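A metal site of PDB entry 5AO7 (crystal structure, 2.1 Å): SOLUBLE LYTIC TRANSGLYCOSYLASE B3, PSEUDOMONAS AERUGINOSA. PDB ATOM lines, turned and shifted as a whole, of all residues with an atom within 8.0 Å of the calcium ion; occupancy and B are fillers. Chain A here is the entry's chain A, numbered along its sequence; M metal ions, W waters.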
ATOM      1  N   ASP A 188       2.069   0.777 -26.101  1.00  0.00           N
ATOM      2  CA  ASP A 188       0.640   0.596 -25.861  1.00  0.00           C
ATOM      3  C   ASP A 188       0.131   1.592 -24.823  1.00  0.00           C
ATOM      4  O   ASP A 188      -1.044   1.989 -24.833  1.00  0.00           O
ATOM      5  CB  ASP A 188       0.323  -0.830 -25.375  1.00  0.00           C
ATOM      6  CG  ASP A 188       0.469  -1.889 -26.471  1.00  0.00           C
ATOM      7  OD1 ASP A 188       0.150  -1.621 -27.667  1.00  0.00           O
ATOM      8  OD2 ASP A 188       0.874  -3.020 -26.120  1.00  0.00           O
ATOM      9  N   VAL A 217      -5.938  -6.711 -27.823  1.00  0.00           N
ATOM     10  CA  VAL A 217      -6.381  -6.319 -29.161  1.00  0.00           C
ATOM     11  C   VAL A 217      -6.357  -4.816 -29.331  1.00  0.00           C
ATOM     12  O   VAL A 217      -6.665  -4.077 -28.379  1.00  0.00           O
ATOM     13  CB  VAL A 217      -7.829  -6.821 -29.404  1.00  0.00           C
ATOM     14  CG1 VAL A 217      -8.439  -6.143 -30.618  1.00  0.00           C
ATOM     15  CG2 VAL A 217      -7.840  -8.357 -29.525  1.00  0.00           C
ATOM     16  N   ASP A 218      -5.996  -4.351 -30.517  1.00  0.00           N
ATOM     17  CA  ASP A 218      -6.198  -2.933 -30.863  1.00  0.00           C
ATOM     18  C   ASP A 218      -7.493  -2.840 -31.651  1.00  0.00           C
ATOM     19  O   ASP A 218      -7.534  -3.106 -32.864  1.00  0.00           O
ATOM     20  CB  ASP A 218      -5.017  -2.396 -31.670  1.00  0.00           C
ATOM     21  CG  ASP A 218      -5.242  -0.996 -32.199  1.00  0.00           C
ATOM     22  OD1 ASP A 218      -6.089  -0.252 -31.649  1.00  0.00           O
ATOM     23  OD2 ASP A 218      -4.553  -0.619 -33.179  1.00  0.00           O
ATOM     24  N   PHE A 219      -8.568  -2.479 -30.957  1.00  0.00           N
ATOM     25  CA  PHE A 219      -9.885  -2.471 -31.547  1.00  0.00           C
ATOM     26  C   PHE A 219     -10.108  -1.269 -32.473  1.00  0.00           C
ATOM     27  O   PHE A 219     -10.665  -1.426 -33.557  1.00  0.00           O
ATOM     28  CB  PHE A 219     -10.944  -2.476 -30.447  1.00  0.00           C
ATOM     29  CG  PHE A 219     -12.345  -2.335 -30.948  1.00  0.00           C
ATOM     30  CD1 PHE A 219     -13.018  -3.435 -31.442  1.00  0.00           C
ATOM     31  CD2 PHE A 219     -12.981  -1.106 -30.939  1.00  0.00           C
ATOM     32  CE1 PHE A 219     -14.313  -3.303 -31.909  1.00  0.00           C
ATOM     33  CE2 PHE A 219     -14.265  -0.982 -31.403  1.00  0.00           C
ATOM     34  CZ  PHE A 219     -14.935  -2.071 -31.883  1.00  0.00           C
ATOM     35  N   ASP A 220      -9.642  -0.094 -32.054  1.00  0.00           N
ATOM     36  CA  ASP A 220      -9.970   1.138 -32.770  1.00  0.00           C
ATOM     37  C   ASP A 220      -8.963   1.502 -33.870  1.00  0.00           C
ATOM     38  O   ASP A 220      -9.217   2.406 -34.660  1.00  0.00           O
ATOM     39  CB  ASP A 220     -10.152   2.300 -31.776  1.00  0.00           C
ATOM     40  CG  ASP A 220      -9.099   2.320 -30.676  1.00  0.00           C
ATOM     41  OD1 ASP A 220      -7.995   1.793 -30.882  1.00  0.00           O
ATOM     42  OD2 ASP A 220      -9.364   2.869 -29.572  1.00  0.00           O
ATOM     43  N   GLY A 221      -7.825   0.816 -33.908  1.00  0.00           N
ATOM     44  CA  GLY A 221      -6.886   0.973 -35.001  1.00  0.00           C
ATOM     45  C   GLY A 221      -5.869   2.093 -34.867  1.00  0.00           C
ATOM     46  O   GLY A 221      -5.261   2.487 -35.856  1.00  0.00           O
ATOM     47  N   ASP A 222      -5.651   2.602 -33.662  1.00  0.00           N
ATOM     48  CA  ASP A 222      -4.650   3.661 -33.492  1.00  0.00           C
ATOM     49  C   ASP A 222      -3.248   3.086 -33.308  1.00  0.00           C
ATOM     50  O   ASP A 222      -2.286   3.836 -33.133  1.00  0.00           O
ATOM     51  CB  ASP A 222      -5.017   4.570 -32.323  1.00  0.00           C
ATOM     52  CG  ASP A 222      -4.958   3.855 -30.985  1.00  0.00           C
ATOM     53  OD1 ASP A 222      -4.928   2.598 -30.967  1.00  0.00           O
ATOM     54  OD2 ASP A 222      -4.955   4.559 -29.955  1.00  0.00           O
ATOM     55  N   GLY A 223      -3.140   1.762 -33.354  1.00  0.00           N
ATOM     56  CA  GLY A 223      -1.857   1.109 -33.178  1.00  0.00           C
ATOM     57  C   GLY A 223      -1.506   0.733 -31.750  1.00  0.00           C
ATOM     58  O   GLY A 223      -0.506   0.067 -31.517  1.00  0.00           O
ATOM     59  N   LYS A 224      -2.328   1.154 -30.784  1.00  0.00           N
ATOM     60  CA  LYS A 224      -2.098   0.821 -29.382  1.00  0.00           C
ATOM     61  C   LYS A 224      -3.098  -0.198 -28.876  1.00  0.00           C
ATOM     62  O   LYS A 224      -4.281  -0.096 -29.154  1.00  0.00           O
ATOM     63  CB  LYS A 224      -2.184   2.082 -28.503  1.00  0.00           C
ATOM     64  CG  LYS A 224      -1.259   3.190 -28.962  1.00  0.00           C
ATOM     65  CD  LYS A 224      -1.104   4.275 -27.893  1.00  0.00           C
ATOM     66  CE  LYS A 224      -2.389   5.010 -27.603  1.00  0.00           C
ATOM     67  NZ  LYS A 224      -2.142   6.091 -26.598  1.00  0.00           N
ATOM     68  N   ARG A 225      -2.599  -1.182 -28.127  1.00  0.00           N
ATOM     69  CA  ARG A 225      -3.482  -2.090 -27.402  1.00  0.00           C
ATOM     70  C   ARG A 225      -3.652  -1.508 -26.019  1.00  0.00           C
ATOM     71  O   ARG A 225      -2.972  -1.919 -25.066  1.00  0.00           O
ATOM     72  CB  ARG A 225      -2.886  -3.494 -27.362  1.00  0.00           C
ATOM     73  CG  ARG A 225      -2.703  -4.013 -28.767  1.00  0.00           C
ATOM     74  CD  ARG A 225      -2.408  -5.495 -28.765  1.00  0.00           C
ATOM     75  NE  ARG A 225      -1.017  -5.769 -28.455  1.00  0.00           N
ATOM     76  CZ  ARG A 225      -0.544  -6.998 -28.209  1.00  0.00           C
ATOM     77  NH1 ARG A 225      -1.359  -8.056 -28.232  1.00  0.00           N
ATOM     78  NH2 ARG A 225       0.736  -7.165 -27.934  1.00  0.00           N
ATOM     79  N   ASP A 226      -4.571  -0.556 -25.920  1.00  0.00           N
ATOM     80  CA  ASP A 226      -4.679   0.265 -24.708  1.00  0.00           C
ATOM     81  C   ASP A 226      -5.766  -0.258 -23.793  1.00  0.00           C
ATOM     82  O   ASP A 226      -6.899   0.206 -23.828  1.00  0.00           O
ATOM     83  CB  ASP A 226      -4.948   1.725 -25.087  1.00  0.00           C
ATOM     84  CG  ASP A 226      -5.119   2.602 -23.858  1.00  0.00           C
ATOM     85  OD1 ASP A 226      -4.725   2.171 -22.755  1.00  0.00           O
ATOM     86  OD2 ASP A 226      -5.644   3.726 -24.002  1.00  0.00           O
ATOM     87  N   ILE A 227      -5.424  -1.218 -22.950  1.00  0.00           N
ATOM     88  CA  ILE A 227      -6.438  -1.791 -22.081  1.00  0.00           C
ATOM     89  C   ILE A 227      -6.641  -0.917 -20.835  1.00  0.00           C
ATOM     90  O   ILE A 227      -7.393  -1.291 -19.939  1.00  0.00           O
ATOM     91  CB  ILE A 227      -6.079  -3.225 -21.648  1.00  0.00           C
ATOM     92  CG1 ILE A 227      -4.740  -3.278 -20.895  1.00  0.00           C
ATOM     93  CG2 ILE A 227      -6.055  -4.135 -22.867  1.00  0.00           C
ATOM     94  CD1 ILE A 227      -4.491  -4.612 -20.133  1.00  0.00           C
ATOM     95  N   SER A 230      -8.841   2.747 -23.274  1.00  0.00           N
ATOM     96  CA  SER A 230      -9.779   2.518 -24.374  1.00  0.00           C
ATOM     97  C   SER A 230     -10.780   1.393 -24.091  1.00  0.00           C
ATOM     98  O   SER A 230     -10.406   0.223 -24.008  1.00  0.00           O
ATOM     99  CB  SER A 230      -9.021   2.187 -25.654  1.00  0.00           C
ATOM    100  OG  SER A 230      -9.908   1.688 -26.631  1.00  0.00           O
ATOM    101  N   GLY A 232     -12.982   0.141 -26.034  1.00  0.00           N
ATOM    102  CA  GLY A 232     -12.975  -0.743 -27.187  1.00  0.00           C
ATOM    103  C   GLY A 232     -11.861  -1.770 -27.133  1.00  0.00           C
ATOM    104  O   GLY A 232     -12.109  -2.958 -27.296  1.00  0.00           O
ATOM    105  N   ASP A 233     -10.637  -1.312 -26.899  1.00  0.00           N
ATOM    106  CA  ASP A 233      -9.500  -2.243 -26.791  1.00  0.00           C
ATOM    107  C   ASP A 233      -9.718  -3.201 -25.628  1.00  0.00           C
ATOM    108  O   ASP A 233      -9.444  -4.397 -25.725  1.00  0.00           O
ATOM    109  CB  ASP A 233      -8.166  -1.522 -26.557  1.00  0.00           C
ATOM    110  CG  ASP A 233      -7.698  -0.671 -27.749  1.00  0.00           C
ATOM    111  OD1 ASP A 233      -8.332  -0.682 -28.838  1.00  0.00           O
ATOM    112  OD2 ASP A 233      -6.678   0.004 -27.582  1.00  0.00           O
ATOM    113  N   ALA A 234     -10.206  -2.672 -24.515  1.00  0.00           N
ATOM    114  CA  ALA A 234     -10.393  -3.506 -23.330  1.00  0.00           C
ATOM    115  C   ALA A 234     -11.414  -4.604 -23.585  1.00  0.00           C
ATOM    116  O   ALA A 234     -11.170  -5.762 -23.249  1.00  0.00           O
ATOM    117  CB  ALA A 234     -10.813  -2.671 -22.144  1.00  0.00           C
HETATM  118 CA    CA M   1      -6.221   1.040 -29.645  1.00  0.00          CA
HETATM  119  O   HOH W   1      -6.185   2.893 -28.227  1.00  0.00           O
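The side-chain carboxylate (OD2) of Asp 218 is in hydrogen-bond range of the backbone NH (N) of Gly 223 (2.8 Å).
N of Gly 221 lies close to OD1 of Asp 218, 3.0 Å away.
OD2 of Asp 220 sits at hydrogen-bond distance from OG of Ser 230 (3.2 Å).
N of Asp 233 sits at hydrogen-bond distance from OG of Ser 230, at 3.1 Å.
N of Phe 219 sits close to OD1 of Asp 233 (2.8 Å).
OD2 of Asp 233 lies close to N of Asp 226 (2.7 Å).
Five residues have an atom within 4 Å of the calcium ion: Asp 218, Asp 220, Asp 222, Lys 224 and Asp 233.
Along chain A the residues within 4 Å of the calcium ion span positions 218 to 233.
The calcium ion is bound by the side-chain carboxylate (OD1) of Asp 220 (2.3 Å), the backbone carbonyl oxygen (O) of Lys 224 (2.3 Å), water W1 (2.3 Å), the side-chain carboxylate (OD2) of Asp 233 (2.4 Å), the side-chain carboxylate (OD1) of Asp 218 (2.4 Å), the side-chain carboxylate (OD1) of Asp 222 (2.4 Å) and the side-chain carboxylate (OD1) of Asp 233 (2.8 Å).
Water W1 bridges the side-chain carboxylate (OD2) of Asp 222 and the side-chain carboxylate (OD2) of Asp 220.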
